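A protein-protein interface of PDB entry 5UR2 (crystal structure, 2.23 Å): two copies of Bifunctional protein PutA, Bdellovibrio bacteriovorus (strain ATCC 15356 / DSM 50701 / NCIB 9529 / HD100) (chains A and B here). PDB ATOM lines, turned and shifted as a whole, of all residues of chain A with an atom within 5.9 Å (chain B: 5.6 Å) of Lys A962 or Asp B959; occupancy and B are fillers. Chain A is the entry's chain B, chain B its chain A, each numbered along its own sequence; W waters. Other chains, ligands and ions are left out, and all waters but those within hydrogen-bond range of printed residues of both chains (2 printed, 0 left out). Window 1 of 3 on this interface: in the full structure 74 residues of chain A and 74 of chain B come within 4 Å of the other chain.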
ATOM      1  N   HIS A 607     -17.054 -21.763  -9.831  1.00  0.00           N
ATOM      2  CA  HIS A 607     -15.720 -22.226  -9.444  1.00  0.00           C
ATOM      3  C   HIS A 607     -14.637 -21.595 -10.316  1.00  0.00           C
ATOM      4  O   HIS A 607     -13.581 -21.194  -9.810  1.00  0.00           O
ATOM      5  CB  HIS A 607     -15.647 -23.752  -9.517  1.00  0.00           C
ATOM      6  CG  HIS A 607     -14.563 -24.356  -8.678  1.00  0.00           C
ATOM      7  ND1 HIS A 607     -14.208 -25.688  -8.768  1.00  0.00           N
ATOM      8  CD2 HIS A 607     -13.763 -23.815  -7.725  1.00  0.00           C
ATOM      9  CE1 HIS A 607     -13.236 -25.939  -7.909  1.00  0.00           C
ATOM     10  NE2 HIS A 607     -12.945 -24.819  -7.268  1.00  0.00           N
ATOM     11  N   LEU A 611     -11.191 -19.718  -9.370  1.00  0.00           N
ATOM     12  CA  LEU A 611      -9.869 -20.227  -9.738  1.00  0.00           C
ATOM     13  C   LEU A 611      -9.116 -19.316 -10.717  1.00  0.00           C
ATOM     14  O   LEU A 611      -7.919 -19.521 -10.921  1.00  0.00           O
ATOM     15  CB  LEU A 611     -10.010 -21.645 -10.321  1.00  0.00           C
ATOM     16  CG  LEU A 611     -10.479 -22.722  -9.319  1.00  0.00           C
ATOM     17  CD1 LEU A 611     -10.714 -24.052  -9.997  1.00  0.00           C
ATOM     18  CD2 LEU A 611      -9.541 -22.913  -8.142  1.00  0.00           C
ATOM     19  N   TYR A 627       0.580 -19.244  -8.041  1.00  0.00           N
ATOM     20  CA  TYR A 627       0.072 -20.544  -8.450  1.00  0.00           C
ATOM     21  C   TYR A 627      -1.216 -20.315  -9.231  1.00  0.00           C
ATOM     22  O   TYR A 627      -2.115 -19.601  -8.760  1.00  0.00           O
ATOM     23  CB  TYR A 627      -0.156 -21.416  -7.209  1.00  0.00           C
ATOM     24  CG  TYR A 627      -0.422 -22.896  -7.415  1.00  0.00           C
ATOM     25  CD1 TYR A 627       0.631 -23.795  -7.596  1.00  0.00           C
ATOM     26  CD2 TYR A 627      -1.712 -23.409  -7.342  1.00  0.00           C
ATOM     27  CE1 TYR A 627       0.399 -25.147  -7.741  1.00  0.00           C
ATOM     28  CE2 TYR A 627      -1.954 -24.766  -7.486  1.00  0.00           C
ATOM     29  CZ  TYR A 627      -0.894 -25.627  -7.678  1.00  0.00           C
ATOM     30  OH  TYR A 627      -1.121 -26.977  -7.817  1.00  0.00           O
ATOM     31  N   TYR A 629      -3.903 -21.875 -12.769  1.00  0.00           N
ATOM     32  CA  TYR A 629      -4.366 -23.016 -13.545  1.00  0.00           C
ATOM     33  C   TYR A 629      -4.421 -22.652 -15.025  1.00  0.00           C
ATOM     34  O   TYR A 629      -4.745 -21.511 -15.382  1.00  0.00           O
ATOM     35  CB  TYR A 629      -5.740 -23.504 -13.065  1.00  0.00           C
ATOM     36  CG  TYR A 629      -5.634 -24.086 -11.686  1.00  0.00           C
ATOM     37  CD1 TYR A 629      -5.219 -25.399 -11.494  1.00  0.00           C
ATOM     38  CD2 TYR A 629      -5.877 -23.301 -10.572  1.00  0.00           C
ATOM     39  CE1 TYR A 629      -5.083 -25.924 -10.213  1.00  0.00           C
ATOM     40  CE2 TYR A 629      -5.741 -23.811  -9.297  1.00  0.00           C
ATOM     41  CZ  TYR A 629      -5.351 -25.115  -9.125  1.00  0.00           C
ATOM     42  OH  TYR A 629      -5.228 -25.596  -7.852  1.00  0.00           O
ATOM     43  N   ARG A 742      -5.356 -37.680 -19.739  1.00  0.00           N
ATOM     44  CA  ARG A 742      -6.005 -37.817 -18.449  1.00  0.00           C
ATOM     45  C   ARG A 742      -7.405 -38.368 -18.649  1.00  0.00           C
ATOM     46  O   ARG A 742      -8.161 -37.857 -19.486  1.00  0.00           O
ATOM     47  CB  ARG A 742      -6.079 -36.490 -17.710  1.00  0.00           C
ATOM     48  CG  ARG A 742      -6.981 -36.605 -16.473  1.00  0.00           C
ATOM     49  CD  ARG A 742      -6.869 -35.409 -15.582  1.00  0.00           C
ATOM     50  NE  ARG A 742      -5.548 -35.338 -14.977  1.00  0.00           N
ATOM     51  CZ  ARG A 742      -4.943 -34.198 -14.663  1.00  0.00           C
ATOM     52  NH1 ARG A 742      -5.549 -33.022 -14.903  1.00  0.00           N
ATOM     53  NH2 ARG A 742      -3.730 -34.238 -14.121  1.00  0.00           N
ATOM     54  N   PRO A 958     -15.410 -29.461  -4.873  1.00  0.00           N
ATOM     55  CA  PRO A 958     -14.352 -28.460  -5.061  1.00  0.00           C
ATOM     56  C   PRO A 958     -13.054 -28.981  -5.682  1.00  0.00           C
ATOM     57  O   PRO A 958     -12.130 -28.182  -5.869  1.00  0.00           O
ATOM     58  CB  PRO A 958     -14.109 -27.965  -3.622  1.00  0.00           C
ATOM     59  CG  PRO A 958     -14.422 -29.178  -2.768  1.00  0.00           C
ATOM     60  CD  PRO A 958     -15.548 -29.889  -3.473  1.00  0.00           C
ATOM     61  N   ASP A 959     -12.935 -30.271  -6.022  1.00  0.00           N
ATOM     62  CA  ASP A 959     -11.752 -30.759  -6.735  1.00  0.00           C
ATOM     63  C   ASP A 959     -12.022 -31.014  -8.210  1.00  0.00           C
ATOM     64  O   ASP A 959     -11.071 -31.247  -8.963  1.00  0.00           O
ATOM     65  CB  ASP A 959     -11.203 -32.060  -6.096  1.00  0.00           C
ATOM     66  CG  ASP A 959     -10.713 -31.854  -4.656  1.00  0.00           C
ATOM     67  OD1 ASP A 959     -10.188 -30.755  -4.343  1.00  0.00           O
ATOM     68  OD2 ASP A 959     -10.901 -32.772  -3.824  1.00  0.00           O
ATOM     69  N   TYR A 960     -13.284 -30.973  -8.646  1.00  0.00           N
ATOM     70  CA  TYR A 960     -13.627 -31.555  -9.944  1.00  0.00           C
ATOM     71  C   TYR A 960     -13.079 -30.738 -11.115  1.00  0.00           C
ATOM     72  O   TYR A 960     -12.472 -31.294 -12.039  1.00  0.00           O
ATOM     73  CB  TYR A 960     -15.131 -31.707 -10.077  1.00  0.00           C
ATOM     74  CG  TYR A 960     -15.515 -32.417 -11.344  1.00  0.00           C
ATOM     75  CD1 TYR A 960     -15.291 -33.786 -11.483  1.00  0.00           C
ATOM     76  CD2 TYR A 960     -16.083 -31.736 -12.395  1.00  0.00           C
ATOM     77  CE1 TYR A 960     -15.634 -34.462 -12.639  1.00  0.00           C
ATOM     78  CE2 TYR A 960     -16.443 -32.404 -13.569  1.00  0.00           C
ATOM     79  CZ  TYR A 960     -16.209 -33.768 -13.681  1.00  0.00           C
ATOM     80  OH  TYR A 960     -16.541 -34.438 -14.828  1.00  0.00           O
ATOM     81  N   LEU A 961     -13.302 -29.423 -11.102  1.00  0.00           N
ATOM     82  CA  LEU A 961     -12.912 -28.578 -12.226  1.00  0.00           C
ATOM     83  C   LEU A 961     -11.406 -28.635 -12.504  1.00  0.00           C
ATOM     84  O   LEU A 961     -10.988 -28.544 -13.671  1.00  0.00           O
ATOM     85  CB  LEU A 961     -13.345 -27.136 -11.958  1.00  0.00           C
ATOM     86  CG  LEU A 961     -13.238 -26.167 -13.128  1.00  0.00           C
ATOM     87  CD1 LEU A 961     -14.032 -26.731 -14.318  1.00  0.00           C
ATOM     88  CD2 LEU A 961     -13.739 -24.780 -12.705  1.00  0.00           C
ATOM     89  N   LYS A 962     -10.585 -28.799 -11.460  1.00  0.00           N
ATOM     90  CA  LYS A 962      -9.132 -28.851 -11.624  1.00  0.00           C
ATOM     91  C   LYS A 962      -8.663 -30.042 -12.455  1.00  0.00           C
ATOM     92  O   LYS A 962      -7.570 -29.987 -13.043  1.00  0.00           O
ATOM     93  CB  LYS A 962      -8.452 -28.889 -10.252  1.00  0.00           C
ATOM     94  CG  LYS A 962      -8.665 -27.611  -9.418  1.00  0.00           C
ATOM     95  CD  LYS A 962      -8.093 -27.800  -8.026  1.00  0.00           C
ATOM     96  CE  LYS A 962      -8.259 -26.566  -7.191  1.00  0.00           C
ATOM     97  NZ  LYS A 962      -7.545 -26.691  -5.895  1.00  0.00           N
ATOM     98  N   GLN A 963      -9.448 -31.117 -12.512  1.00  0.00           N
ATOM     99  CA  GLN A 963      -9.088 -32.268 -13.344  1.00  0.00           C
ATOM    100  C   GLN A 963      -9.024 -31.909 -14.825  1.00  0.00           C
ATOM    101  O   GLN A 963      -8.388 -32.628 -15.605  1.00  0.00           O
ATOM    102  CB  GLN A 963     -10.099 -33.397 -13.137  1.00  0.00           C
ATOM    103  CG  GLN A 963     -10.033 -34.090 -11.780  1.00  0.00           C
ATOM    104  CD  GLN A 963      -8.851 -35.029 -11.688  1.00  0.00           C
ATOM    105  OE1 GLN A 963      -7.760 -34.633 -11.282  1.00  0.00           O
ATOM    106  NE2 GLN A 963      -9.045 -36.271 -12.129  1.00  0.00           N
ATOM    107  N   TYR A 964      -9.710 -30.842 -15.230  1.00  0.00           N
ATOM    108  CA  TYR A 964      -9.704 -30.365 -16.603  1.00  0.00           C
ATOM    109  C   TYR A 964      -8.625 -29.318 -16.849  1.00  0.00           C
ATOM    110  O   TYR A 964      -8.619 -28.700 -17.918  1.00  0.00           O
ATOM    111  CB  TYR A 964     -11.082 -29.783 -16.962  1.00  0.00           C
ATOM    112  CG  TYR A 964     -12.174 -30.832 -16.964  1.00  0.00           C
ATOM    113  CD1 TYR A 964     -12.850 -31.175 -15.794  1.00  0.00           C
ATOM    114  CD2 TYR A 964     -12.511 -31.491 -18.137  1.00  0.00           C
ATOM    115  CE1 TYR A 964     -13.851 -32.148 -15.803  1.00  0.00           C
ATOM    116  CE2 TYR A 964     -13.502 -32.443 -18.164  1.00  0.00           C
ATOM    117  CZ  TYR A 964     -14.171 -32.771 -17.001  1.00  0.00           C
ATOM    118  OH  TYR A 964     -15.145 -33.738 -17.074  1.00  0.00           O
ATOM    119  N   MET A 965      -7.701 -29.132 -15.902  1.00  0.00           N
ATOM    120  CA  MET A 965      -6.708 -28.068 -15.959  1.00  0.00           C
ATOM    121  C   MET A 965      -5.352 -28.631 -15.553  1.00  0.00           C
ATOM    122  O   MET A 965      -5.240 -29.783 -15.128  1.00  0.00           O
ATOM    123  CB  MET A 965      -7.118 -26.870 -15.068  1.00  0.00           C
ATOM    124  CG  MET A 965      -8.420 -26.244 -15.536  1.00  0.00           C
ATOM    125  SD  MET A 965      -8.906 -24.713 -14.697  1.00  0.00           S
ATOM    126  CE  MET A 965      -8.932 -25.254 -13.003  1.00  0.00           C
ATOM    127  N   GLU A 966      -4.307 -27.819 -15.753  1.00  0.00           N
ATOM    128  CA  GLU A 966      -2.959 -28.053 -15.272  1.00  0.00           C
ATOM    129  C   GLU A 966      -2.580 -26.962 -14.282  1.00  0.00           C
ATOM    130  O   GLU A 966      -2.808 -25.777 -14.551  1.00  0.00           O
ATOM    131  CB  GLU A 966      -1.909 -28.066 -16.411  1.00  0.00           C
ATOM    132  CG  GLU A 966      -1.942 -29.269 -17.327  1.00  0.00           C
ATOM    133  CD  GLU A 966      -1.508 -30.521 -16.635  1.00  0.00           C
ATOM    134  OE1 GLU A 966      -0.606 -30.433 -15.760  1.00  0.00           O
ATOM    135  OE2 GLU A 966      -2.075 -31.594 -16.958  1.00  0.00           O
ATOM    136  N   PRO A 967      -1.980 -27.322 -13.155  1.00  0.00           N
ATOM    137  CA  PRO A 967      -1.433 -26.299 -12.260  1.00  0.00           C
ATOM    138  C   PRO A 967      -0.151 -25.735 -12.842  1.00  0.00           C
ATOM    139  O   PRO A 967       0.604 -26.438 -13.521  1.00  0.00           O
ATOM    140  CB  PRO A 967      -1.143 -27.080 -10.975  1.00  0.00           C
ATOM    141  CG  PRO A 967      -0.744 -28.474 -11.515  1.00  0.00           C
ATOM    142  CD  PRO A 967      -1.633 -28.698 -12.722  1.00  0.00           C
ATOM    143  N   HIS B 607       0.151 -29.668   5.640  1.00  0.00           N
ATOM    144  CA  HIS B 607      -1.013 -29.803   4.768  1.00  0.00           C
ATOM    145  C   HIS B 607      -1.982 -30.863   5.297  1.00  0.00           C
ATOM    146  O   HIS B 607      -3.204 -30.659   5.311  1.00  0.00           O
ATOM    147  CB  HIS B 607      -0.553 -30.150   3.345  1.00  0.00           C
ATOM    148  CG  HIS B 607      -1.558 -29.819   2.288  1.00  0.00           C
ATOM    149  ND1 HIS B 607      -2.751 -29.184   2.569  1.00  0.00           N
ATOM    150  CD2 HIS B 607      -1.538 -30.007   0.949  1.00  0.00           C
ATOM    151  CE1 HIS B 607      -3.426 -29.001   1.448  1.00  0.00           C
ATOM    152  NE2 HIS B 607      -2.712 -29.491   0.450  1.00  0.00           N
ATOM    153  N   LYS B 954       2.707 -31.898  -9.039  1.00  0.00           N
ATOM    154  CA  LYS B 954       3.020 -30.502  -8.764  1.00  0.00           C
ATOM    155  C   LYS B 954       3.472 -30.435  -7.312  1.00  0.00           C
ATOM    156  O   LYS B 954       2.694 -30.047  -6.433  1.00  0.00           O
ATOM    157  CB  LYS B 954       1.810 -29.593  -9.043  1.00  0.00           C
ATOM    158  CG  LYS B 954       2.165 -28.097  -9.121  1.00  0.00           C
ATOM    159  CD  LYS B 954       3.235 -27.852 -10.184  1.00  0.00           C
ATOM    160  CE  LYS B 954       3.145 -26.436 -10.742  1.00  0.00           C
ATOM    161  NZ  LYS B 954       4.408 -26.100 -11.472  1.00  0.00           N
ATOM    162  N   GLY B 957       3.230 -27.949  -3.523  1.00  0.00           N
ATOM    163  CA  GLY B 957       2.120 -27.041  -3.727  1.00  0.00           C
ATOM    164  C   GLY B 957       0.828 -27.597  -3.158  1.00  0.00           C
ATOM    165  O   GLY B 957       0.767 -28.745  -2.701  1.00  0.00           O
ATOM    166  N   PRO B 958      -0.241 -26.797  -3.185  1.00  0.00           N
ATOM    167  CA  PRO B 958      -1.454 -27.160  -2.438  1.00  0.00           C
ATOM    168  C   PRO B 958      -2.313 -28.231  -3.092  1.00  0.00           C
ATOM    169  O   PRO B 958      -3.342 -28.596  -2.513  1.00  0.00           O
ATOM    170  CB  PRO B 958      -2.225 -25.829  -2.356  1.00  0.00           C
ATOM    171  CG  PRO B 958      -1.818 -25.096  -3.596  1.00  0.00           C
ATOM    172  CD  PRO B 958      -0.360 -25.484  -3.835  1.00  0.00           C
ATOM    173  N   ASP B 959      -1.938 -28.767  -4.256  1.00  0.00           N
ATOM    174  CA  ASP B 959      -2.703 -29.858  -4.839  1.00  0.00           C
ATOM    175  C   ASP B 959      -2.035 -31.218  -4.673  1.00  0.00           C
ATOM    176  O   ASP B 959      -2.699 -32.240  -4.888  1.00  0.00           O
ATOM    177  CB  ASP B 959      -2.952 -29.602  -6.335  1.00  0.00           C
ATOM    178  CG  ASP B 959      -3.823 -28.376  -6.583  1.00  0.00           C
ATOM    179  OD1 ASP B 959      -4.715 -28.099  -5.743  1.00  0.00           O
ATOM    180  OD2 ASP B 959      -3.607 -27.691  -7.613  1.00  0.00           O
ATOM    181  N   TYR B 960      -0.768 -31.257  -4.242  1.00  0.00           N
ATOM    182  CA  TYR B 960       0.040 -32.466  -4.386  1.00  0.00           C
ATOM    183  C   TYR B 960      -0.446 -33.593  -3.481  1.00  0.00           C
ATOM    184  O   TYR B 960      -0.660 -34.722  -3.942  1.00  0.00           O
ATOM    185  CB  TYR B 960       1.508 -32.159  -4.088  1.00  0.00           C
ATOM    186  CG  TYR B 960       2.404 -33.340  -4.365  1.00  0.00           C
ATOM    187  CD1 TYR B 960       2.648 -33.741  -5.674  1.00  0.00           C
ATOM    188  CD2 TYR B 960       3.006 -34.047  -3.333  1.00  0.00           C
ATOM    189  CE1 TYR B 960       3.472 -34.810  -5.960  1.00  0.00           C
ATOM    190  CE2 TYR B 960       3.823 -35.137  -3.606  1.00  0.00           C
ATOM    191  CZ  TYR B 960       4.063 -35.504  -4.924  1.00  0.00           C
ATOM    192  OH  TYR B 960       4.886 -36.581  -5.225  1.00  0.00           O
ATOM    193  N   LEU B 961      -0.648 -33.302  -2.194  1.00  0.00           N
ATOM    194  CA  LEU B 961      -0.996 -34.350  -1.236  1.00  0.00           C
ATOM    195  C   LEU B 961      -2.299 -35.057  -1.611  1.00  0.00           C
ATOM    196  O   LEU B 961      -2.453 -36.255  -1.347  1.00  0.00           O
ATOM    197  CB  LEU B 961      -1.076 -33.742   0.176  1.00  0.00           C
ATOM    198  CG  LEU B 961      -1.221 -34.662   1.390  1.00  0.00           C
ATOM    199  CD1 LEU B 961      -0.130 -35.717   1.399  1.00  0.00           C
ATOM    200  CD2 LEU B 961      -1.203 -33.843   2.720  1.00  0.00           C
ATOM    201  N   LYS B 962      -3.243 -34.341  -2.227  1.00  0.00           N
ATOM    202  CA  LYS B 962      -4.515 -34.950  -2.581  1.00  0.00           C
ATOM    203  C   LYS B 962      -4.362 -36.062  -3.602  1.00  0.00           C
ATOM    204  O   LYS B 962      -5.213 -36.954  -3.656  1.00  0.00           O
ATOM    205  CB  LYS B 962      -5.476 -33.891  -3.105  1.00  0.00           C
ATOM    206  CG  LYS B 962      -5.862 -32.868  -2.040  1.00  0.00           C
ATOM    207  CD  LYS B 962      -6.736 -31.767  -2.640  1.00  0.00           C
ATOM    208  CE  LYS B 962      -7.114 -30.712  -1.609  1.00  0.00           C
ATOM    209  NZ  LYS B 962      -8.096 -29.751  -2.205  1.00  0.00           N
ATOM    210  N   GLN B 963      -3.287 -36.043  -4.389  1.00  0.00           N
ATOM    211  CA  GLN B 963      -3.052 -37.116  -5.339  1.00  0.00           C
ATOM    212  C   GLN B 963      -2.885 -38.462  -4.652  1.00  0.00           C
ATOM    213  O   GLN B 963      -3.122 -39.503  -5.277  1.00  0.00           O
ATOM    214  CB  GLN B 963      -1.812 -36.791  -6.175  1.00  0.00           C
ATOM    215  CG  GLN B 963      -2.053 -35.634  -7.125  1.00  0.00           C
ATOM    216  CD  GLN B 963      -2.917 -36.061  -8.281  1.00  0.00           C
ATOM    217  OE1 GLN B 963      -4.136 -36.015  -8.197  1.00  0.00           O
ATOM    218  NE2 GLN B 963      -2.290 -36.506  -9.363  1.00  0.00           N
HETATM  219  O   HOH W   1      -6.061 -27.911  -3.005  1.00  0.00           O
HETATM  220  O   HOH W   2       0.487 -28.587  -5.970  1.00  0.00           O
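The backbone carbonyl oxygen (O) of Pro B958 sits at hydrogen-bond distance from a ring nitrogen (NE2) of His B607.
OH of Tyr A629 is in hydrogen-bond range of NZ of Lys A962, at 3.2 Å.
CG of Lys B954 touches CE1 of Tyr A627 (3.7 Å).
Pro B958 touches Tyr A627 (CD to CZ, 3.9 Å).
Pro A967 touches Lys B954 (CG to CB, 3.7 Å).
Printed residues of chain B that touch a printed residue of chain A: Lys B954, Pro B958, Asp B959 and Lys B962.
Among the printed residues, Asp or Glu carboxylates within 4 Å of a Lys or Arg side-chain nitrogen of the other chain: Asp A959 with Lys B962 and Lys A962 with Asp B959.
Printed residues of chain B within 4 Å of Lys A962: Asp B959.
Asp B959 touches just these residues of chain A: Tyr A627, Tyr A629 and Lys A962.
Of the printed residues of chain A, Lys B954 touches Tyr A627 and Pro A967.
Printed residues of chain A within 4 Å of Lys B962: Asp A959.
Of the printed residues of chain A, Pro B958 touches Tyr A627.
Of the printed residues of chain B, Asp A959 touches Lys B962.
The nearest printed residue of chain B that does not touch Tyr A629 is Pro B958 (5.5 Å).
Water W2 lies within hydrogen-bond range of O of Lys B954 (2.7 Å), OH of Tyr A627 (2.9 Å), N of Asp B959 (3.0 Å), O of Gly B957 (3.3 Å) and N of Tyr B960 (3.4 Å).
Water W1 lies within hydrogen-bond range of O of Pro B958, NZ of Lys B962, OD1 of Asp B959 and NZ of Lys A962.
Asp A959 touches Lys B962, and with the chains exchanged Lys A962 touches Asp B959.
OD2 of Asp B959 sits at hydrogen-bond distance from OH of Tyr A627 (2.6 Å).
OH of Tyr A629 is in hydrogen-bond range of OD2 of Asp B959 (2.7 Å).
OD1 of Asp B959 lies within salt-bridge range of NZ of Lys A962 (3.2 Å).
The side-chain amino group of Lys B962 lies within salt-bridge range of the side-chain carboxylate of Asp A959 (3.2 Å).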
